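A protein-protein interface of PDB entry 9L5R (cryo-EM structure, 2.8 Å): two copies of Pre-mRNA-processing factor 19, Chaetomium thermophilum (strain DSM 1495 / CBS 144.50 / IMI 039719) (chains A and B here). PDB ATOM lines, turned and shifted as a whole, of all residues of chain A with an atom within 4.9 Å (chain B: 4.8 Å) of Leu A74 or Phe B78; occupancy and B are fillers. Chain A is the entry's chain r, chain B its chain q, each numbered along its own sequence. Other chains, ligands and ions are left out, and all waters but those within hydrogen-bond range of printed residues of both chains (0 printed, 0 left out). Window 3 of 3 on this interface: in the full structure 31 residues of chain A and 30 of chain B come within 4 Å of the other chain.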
ATOM      1  N   ARG A  64      14.762 -20.333   8.304  1.00  0.00           N
ATOM      2  CA  ARG A  64      13.321 -20.118   8.323  1.00  0.00           C
ATOM      3  C   ARG A  64      12.886 -19.631   9.701  1.00  0.00           C
ATOM      4  O   ARG A  64      13.218 -20.263  10.710  1.00  0.00           O
ATOM      5  CB  ARG A  64      12.604 -21.415   7.961  1.00  0.00           C
ATOM      6  CG  ARG A  64      11.127 -21.276   7.658  1.00  0.00           C
ATOM      7  CD  ARG A  64      10.524 -22.638   7.350  1.00  0.00           C
ATOM      8  NE  ARG A  64       9.126 -22.550   6.949  1.00  0.00           N
ATOM      9  CZ  ARG A  64       8.698 -22.629   5.698  1.00  0.00           C
ATOM     10  NH1 ARG A  64       9.537 -22.808   4.690  1.00  0.00           N
ATOM     11  NH2 ARG A  64       7.395 -22.529   5.450  1.00  0.00           N
ATOM     12  N   PHE A  68       7.040 -17.948  10.005  1.00  0.00           N
ATOM     13  CA  PHE A  68       6.840 -18.233   8.584  1.00  0.00           C
ATOM     14  C   PHE A  68       7.029 -19.716   8.278  1.00  0.00           C
ATOM     15  O   PHE A  68       7.856 -20.101   7.454  1.00  0.00           O
ATOM     16  CB  PHE A  68       7.786 -17.375   7.753  1.00  0.00           C
ATOM     17  CG  PHE A  68       7.473 -15.900   7.791  1.00  0.00           C
ATOM     18  CD1 PHE A  68       6.253 -15.437   8.267  1.00  0.00           C
ATOM     19  CD2 PHE A  68       8.419 -14.973   7.384  1.00  0.00           C
ATOM     20  CE1 PHE A  68       5.979 -14.083   8.315  1.00  0.00           C
ATOM     21  CE2 PHE A  68       8.151 -13.617   7.432  1.00  0.00           C
ATOM     22  CZ  PHE A  68       6.929 -13.172   7.899  1.00  0.00           C
ATOM     23  N   SER A  70       4.038 -21.846   7.883  1.00  0.00           N
ATOM     24  CA  SER A  70       2.885 -22.267   7.105  1.00  0.00           C
ATOM     25  C   SER A  70       2.864 -21.544   5.763  1.00  0.00           C
ATOM     26  O   SER A  70       3.455 -20.475   5.595  1.00  0.00           O
ATOM     27  CB  SER A  70       1.584 -21.998   7.865  1.00  0.00           C
ATOM     28  OG  SER A  70       1.250 -20.623   7.833  1.00  0.00           O
ATOM     29  N   ILE A  71       2.184 -22.169   4.796  1.00  0.00           N
ATOM     30  CA  ILE A  71       2.010 -21.538   3.482  1.00  0.00           C
ATOM     31  C   ILE A  71       1.258 -20.212   3.551  1.00  0.00           C
ATOM     32  O   ILE A  71       1.671 -19.269   2.859  1.00  0.00           O
ATOM     33  CB  ILE A  71       1.398 -22.539   2.493  1.00  0.00           C
ATOM     34  CG1 ILE A  71       2.176 -23.856   2.521  1.00  0.00           C
ATOM     35  CG2 ILE A  71       1.391 -21.974   1.079  1.00  0.00           C
ATOM     36  CD1 ILE A  71       3.623 -23.720   2.096  1.00  0.00           C
ATOM     37  N   PRO A  72       0.160 -20.054   4.317  1.00  0.00           N
ATOM     38  CA  PRO A  72      -0.423 -18.702   4.449  1.00  0.00           C
ATOM     39  C   PRO A  72       0.509 -17.672   5.069  1.00  0.00           C
ATOM     40  O   PRO A  72       0.443 -16.492   4.696  1.00  0.00           O
ATOM     41  CB  PRO A  72      -1.655 -18.940   5.331  1.00  0.00           C
ATOM     42  CG  PRO A  72      -2.042 -20.321   5.043  1.00  0.00           C
ATOM     43  CD  PRO A  72      -0.750 -21.056   4.918  1.00  0.00           C
ATOM     44  N   SER A  73       1.367 -18.078   6.007  1.00  0.00           N
ATOM     45  CA  SER A  73       2.349 -17.151   6.562  1.00  0.00           C
ATOM     46  C   SER A  73       3.352 -16.713   5.501  1.00  0.00           C
ATOM     47  O   SER A  73       3.701 -15.528   5.418  1.00  0.00           O
ATOM     48  CB  SER A  73       3.068 -17.795   7.747  1.00  0.00           C
ATOM     49  OG  SER A  73       3.809 -18.928   7.333  1.00  0.00           O
ATOM     50  N   LEU A  74       3.810 -17.654   4.671  1.00  0.00           N
ATOM     51  CA  LEU A  74       4.689 -17.304   3.561  1.00  0.00           C
ATOM     52  C   LEU A  74       3.989 -16.400   2.557  1.00  0.00           C
ATOM     53  O   LEU A  74       4.615 -15.498   1.995  1.00  0.00           O
ATOM     54  CB  LEU A  74       5.196 -18.568   2.867  1.00  0.00           C
ATOM     55  CG  LEU A  74       6.047 -19.559   3.665  1.00  0.00           C
ATOM     56  CD1 LEU A  74       6.589 -20.641   2.745  1.00  0.00           C
ATOM     57  CD2 LEU A  74       7.182 -18.847   4.377  1.00  0.00           C
ATOM     58  N   LEU A  75       2.687 -16.603   2.344  1.00  0.00           N
ATOM     59  CA  LEU A  75       1.959 -15.767   1.395  1.00  0.00           C
ATOM     60  C   LEU A  75       1.771 -14.347   1.922  1.00  0.00           C
ATOM     61  O   LEU A  75       1.925 -13.375   1.170  1.00  0.00           O
ATOM     62  CB  LEU A  75       0.614 -16.413   1.066  1.00  0.00           C
ATOM     63  CG  LEU A  75       0.729 -17.637   0.153  1.00  0.00           C
ATOM     64  CD1 LEU A  75      -0.617 -18.322  -0.027  1.00  0.00           C
ATOM     65  CD2 LEU A  75       1.330 -17.255  -1.193  1.00  0.00           C
ATOM     66  N   LYS A  76       1.434 -14.197   3.206  1.00  0.00           N
ATOM     67  CA  LYS A  76       1.304 -12.845   3.747  1.00  0.00           C
ATOM     68  C   LYS A  76       2.660 -12.152   3.829  1.00  0.00           C
ATOM     69  O   LYS A  76       2.740 -10.933   3.632  1.00  0.00           O
ATOM     70  CB  LYS A  76       0.598 -12.863   5.107  1.00  0.00           C
ATOM     71  CG  LYS A  76       1.346 -13.525   6.246  1.00  0.00           C
ATOM     72  CD  LYS A  76       0.645 -13.294   7.572  1.00  0.00           C
ATOM     73  CE  LYS A  76      -0.684 -14.030   7.628  1.00  0.00           C
ATOM     74  NZ  LYS A  76      -0.500 -15.508   7.645  1.00  0.00           N
ATOM     75  N   ALA A  77       3.736 -12.914   4.064  1.00  0.00           N
ATOM     76  CA  ALA A  77       5.078 -12.352   3.957  1.00  0.00           C
ATOM     77  C   ALA A  77       5.380 -11.917   2.529  1.00  0.00           C
ATOM     78  O   ALA A  77       6.044 -10.898   2.311  1.00  0.00           O
ATOM     79  CB  ALA A  77       6.111 -13.371   4.432  1.00  0.00           C
ATOM     80  N   PHE A  78       4.900 -12.687   1.548  1.00  0.00           N
ATOM     81  CA  PHE A  78       5.079 -12.341   0.141  1.00  0.00           C
ATOM     82  C   PHE A  78       4.420 -11.007  -0.182  1.00  0.00           C
ATOM     83  O   PHE A  78       5.046 -10.119  -0.776  1.00  0.00           O
ATOM     84  CB  PHE A  78       4.502 -13.461  -0.728  1.00  0.00           C
ATOM     85  CG  PHE A  78       5.193 -13.641  -2.044  1.00  0.00           C
ATOM     86  CD1 PHE A  78       6.515 -14.049  -2.096  1.00  0.00           C
ATOM     87  CD2 PHE A  78       4.509 -13.440  -3.230  1.00  0.00           C
ATOM     88  CE1 PHE A  78       7.150 -14.229  -3.309  1.00  0.00           C
ATOM     89  CE2 PHE A  78       5.138 -13.622  -4.447  1.00  0.00           C
ATOM     90  CZ  PHE A  78       6.461 -14.014  -4.486  1.00  0.00           C
ATOM     91  N   PHE B  68      15.140 -15.019   5.330  1.00  0.00           N
ATOM     92  CA  PHE B  68      14.162 -15.916   4.724  1.00  0.00           C
ATOM     93  C   PHE B  68      12.884 -15.202   4.308  1.00  0.00           C
ATOM     94  O   PHE B  68      12.159 -15.712   3.448  1.00  0.00           O
ATOM     95  CB  PHE B  68      13.822 -17.046   5.695  1.00  0.00           C
ATOM     96  CG  PHE B  68      13.228 -18.256   5.039  1.00  0.00           C
ATOM     97  CD1 PHE B  68      14.037 -19.183   4.404  1.00  0.00           C
ATOM     98  CD2 PHE B  68      11.860 -18.475   5.070  1.00  0.00           C
ATOM     99  CE1 PHE B  68      13.492 -20.304   3.803  1.00  0.00           C
ATOM    100  CE2 PHE B  68      11.308 -19.591   4.470  1.00  0.00           C
ATOM    101  CZ  PHE B  68      12.126 -20.507   3.838  1.00  0.00           C
ATOM    102  N   LEU B  74      11.647 -16.466  -0.513  1.00  0.00           N
ATOM    103  CA  LEU B  74      10.279 -16.972  -0.488  1.00  0.00           C
ATOM    104  C   LEU B  74       9.952 -17.769  -1.745  1.00  0.00           C
ATOM    105  O   LEU B  74       9.270 -18.794  -1.671  1.00  0.00           O
ATOM    106  CB  LEU B  74       9.298 -15.817  -0.301  1.00  0.00           C
ATOM    107  CG  LEU B  74       9.186 -15.278   1.129  1.00  0.00           C
ATOM    108  CD1 LEU B  74       7.982 -14.369   1.269  1.00  0.00           C
ATOM    109  CD2 LEU B  74       9.122 -16.412   2.145  1.00  0.00           C
ATOM    110  N   LEU B  75      10.441 -17.330  -2.907  1.00  0.00           N
ATOM    111  CA  LEU B  75      10.186 -18.083  -4.130  1.00  0.00           C
ATOM    112  C   LEU B  75      11.025 -19.351  -4.196  1.00  0.00           C
ATOM    113  O   LEU B  75      10.565 -20.359  -4.747  1.00  0.00           O
ATOM    114  CB  LEU B  75      10.419 -17.209  -5.368  1.00  0.00           C
ATOM    115  CG  LEU B  75      11.791 -16.675  -5.791  1.00  0.00           C
ATOM    116  CD1 LEU B  75      12.480 -17.603  -6.784  1.00  0.00           C
ATOM    117  CD2 LEU B  75      11.642 -15.286  -6.392  1.00  0.00           C
ATOM    118  N   LYS B  76      12.243 -19.332  -3.640  1.00  0.00           N
ATOM    119  CA  LYS B  76      13.003 -20.573  -3.521  1.00  0.00           C
ATOM    120  C   LYS B  76      12.303 -21.554  -2.588  1.00  0.00           C
ATOM    121  O   LYS B  76      12.269 -22.761  -2.856  1.00  0.00           O
ATOM    122  CB  LYS B  76      14.425 -20.280  -3.045  1.00  0.00           C
ATOM    123  CG  LYS B  76      15.459 -20.327  -4.163  1.00  0.00           C
ATOM    124  CD  LYS B  76      15.384 -19.079  -5.026  1.00  0.00           C
ATOM    125  CE  LYS B  76      16.458 -19.061  -6.097  1.00  0.00           C
ATOM    126  NZ  LYS B  76      16.340 -17.863  -6.976  1.00  0.00           N
ATOM    127  N   ALA B  77      11.713 -21.048  -1.501  1.00  0.00           N
ATOM    128  CA  ALA B  77      10.923 -21.894  -0.612  1.00  0.00           C
ATOM    129  C   ALA B  77       9.684 -22.436  -1.313  1.00  0.00           C
ATOM    130  O   ALA B  77       9.315 -23.599  -1.119  1.00  0.00           O
ATOM    131  CB  ALA B  77      10.531 -21.114   0.641  1.00  0.00           C
ATOM    132  N   PHE B  78       9.027 -21.603  -2.129  1.00  0.00           N
ATOM    133  CA  PHE B  78       7.860 -22.054  -2.883  1.00  0.00           C
ATOM    134  C   PHE B  78       8.219 -23.158  -3.867  1.00  0.00           C
ATOM    135  O   PHE B  78       7.518 -24.172  -3.944  1.00  0.00           O
ATOM    136  CB  PHE B  78       7.205 -20.887  -3.626  1.00  0.00           C
ATOM    137  CG  PHE B  78       6.538 -19.873  -2.733  1.00  0.00           C
ATOM    138  CD1 PHE B  78       6.266 -20.157  -1.403  1.00  0.00           C
ATOM    139  CD2 PHE B  78       6.167 -18.636  -3.238  1.00  0.00           C
ATOM    140  CE1 PHE B  78       5.644 -19.223  -0.595  1.00  0.00           C
ATOM    141  CE2 PHE B  78       5.546 -17.698  -2.433  1.00  0.00           C
ATOM    142  CZ  PHE B  78       5.285 -17.993  -1.109  1.00  0.00           C
ATOM    143  N   GLN B  79       9.312 -22.994  -4.618  1.00  0.00           N
ATOM    144  CA  GLN B  79       9.664 -24.027  -5.587  1.00  0.00           C
ATOM    145  C   GLN B  79      10.191 -25.284  -4.904  1.00  0.00           C
ATOM    146  O   GLN B  79       9.957 -26.390  -5.397  1.00  0.00           O
ATOM    147  CB  GLN B  79      10.667 -23.502  -6.619  1.00  0.00           C
ATOM    148  CG  GLN B  79      11.971 -22.966  -6.073  1.00  0.00           C
ATOM    149  CD  GLN B  79      13.057 -24.018  -5.983  1.00  0.00           C
ATOM    150  OE1 GLN B  79      13.048 -25.000  -6.723  1.00  0.00           O
ATOM    151  NE2 GLN B  79      14.003 -23.814  -5.074  1.00  0.00           N
ATOM    152  N   ASP B  80      10.860 -25.148  -3.754  1.00  0.00           N
ATOM    153  CA  ASP B  80      11.301 -26.332  -3.021  1.00  0.00           C
ATOM    154  C   ASP B  80      10.120 -27.092  -2.424  1.00  0.00           C
ATOM    155  O   ASP B  80      10.082 -28.329  -2.469  1.00  0.00           O
ATOM    156  CB  ASP B  80      12.291 -25.932  -1.929  1.00  0.00           C
ATOM    157  CG  ASP B  80      13.695 -25.731  -2.463  1.00  0.00           C
ATOM    158  OD1 ASP B  80      14.086 -26.465  -3.396  1.00  0.00           O
ATOM    159  OD2 ASP B  80      14.407 -24.840  -1.953  1.00  0.00           O
ATOM    160  N   GLU B  81       9.144 -26.369  -1.865  1.00  0.00           N
ATOM    161  CA  GLU B  81       7.953 -27.016  -1.329  1.00  0.00           C
ATOM    162  C   GLU B  81       7.122 -27.643  -2.439  1.00  0.00           C
ATOM    163  O   GLU B  81       6.552 -28.724  -2.256  1.00  0.00           O
ATOM    164  CB  GLU B  81       7.124 -26.010  -0.530  1.00  0.00           C
ATOM    165  CG  GLU B  81       5.887 -26.602   0.126  1.00  0.00           C
ATOM    166  CD  GLU B  81       6.218 -27.710   1.107  1.00  0.00           C
ATOM    167  OE1 GLU B  81       7.251 -27.608   1.801  1.00  0.00           O
ATOM    168  OE2 GLU B  81       5.447 -28.689   1.180  1.00  0.00           O
ATOM    169  N   TRP B  82       7.049 -26.984  -3.598  1.00  0.00           N
ATOM    170  CA  TRP B  82       6.371 -27.568  -4.748  1.00  0.00           C
ATOM    171  C   TRP B  82       7.087 -28.823  -5.223  1.00  0.00           C
ATOM    172  O   TRP B  82       6.440 -29.811  -5.573  1.00  0.00           O
ATOM    173  CB  TRP B  82       6.271 -26.542  -5.875  1.00  0.00           C
ATOM    174  CG  TRP B  82       5.567 -27.045  -7.100  1.00  0.00           C
ATOM    175  CD1 TRP B  82       4.221 -27.064  -7.320  1.00  0.00           C
ATOM    176  CD2 TRP B  82       6.174 -27.589  -8.278  1.00  0.00           C
ATOM    177  NE1 TRP B  82       3.951 -27.590  -8.559  1.00  0.00           N
ATOM    178  CE2 TRP B  82       5.133 -27.919  -9.169  1.00  0.00           C
ATOM    179  CE3 TRP B  82       7.496 -27.831  -8.666  1.00  0.00           C
ATOM    180  CZ2 TRP B  82       5.373 -28.482 -10.421  1.00  0.00           C
ATOM    181  CZ3 TRP B  82       7.731 -28.389  -9.911  1.00  0.00           C
ATOM    182  CH2 TRP B  82       6.675 -28.708 -10.772  1.00  0.00           C
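Phe B78 touches two residues of chain A.
Printed residues of chain A within 4 Å of Phe B68: Arg A64 (3.6 Å).
Of the printed residues of chain A, Leu B74 touches Leu A74 (3.6 Å), Ala A77 (3.8 Å) and Phe A78 (3.5 Å).
Of the printed residues of chain B, Ala A77 touches Leu B74 (3.8 Å).
Of the printed residues of chain B, Phe A78 touches Leu B74 (3.5 Å) and Phe B78 (3.8 Å).
Of the printed residues of chain B, Arg A64 touches Phe B68.
Pro A72 touches none of the printed residues of chain B.
Lys A76 touches none of the printed residues of chain B.
The nearest residue of chain B that does not touch Leu A74 is Phe B68 (4.2 Å).
Of the 11 printed residues of chain A, 4 touch a printed residue of chain B.
Hydrophobic or aromatic side chains of chain A within 4 Å of the printed part of chain B: Leu A74, Ala A77 and Phe A78.
Printed residues of chain B that touch a printed residue of chain A: Phe B68, Leu B74 and Phe B78.
Among the printed residues, 6 pairs touch across the chains.
Among the printed residues, no Asp or Glu carboxylate lies within 4 Å of a Lys or Arg side-chain nitrogen of the other chain.
O of Phe A68 lies within hydrogen-bond range of NE of Arg A64 (2.8 Å).
Among the printed residues, pairs that only touch across the chains: Arg A64 with Phe B68 (3.6 Å), Leu A74 with Leu B74 (3.6 Å), Leu A74 with Phe B78 (3.6 Å), Ala A77 with Leu B74 (3.8 Å), Phe A78 with Leu B74 (3.5 Å) and Phe A78 with Phe B78 (3.8 Å).
Leu B74 touches its own counterpart, Leu A74.
Leu A74 touches Phe B78, and with the chains exchanged Phe A78 touches Leu B74.
Ala A77 touches Leu B74, but with the chains exchanged Leu A74 does not touch Ala B77 (4.5 Å).
Phe A78 touches its own counterpart, Phe B78.
Positions printed for both chains: 68, 74, 75, 76, 77 and 78.
Of the 6 pairs that touch across the chains among the printed residues, 4 have their exchanged pair printed and touching as well.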
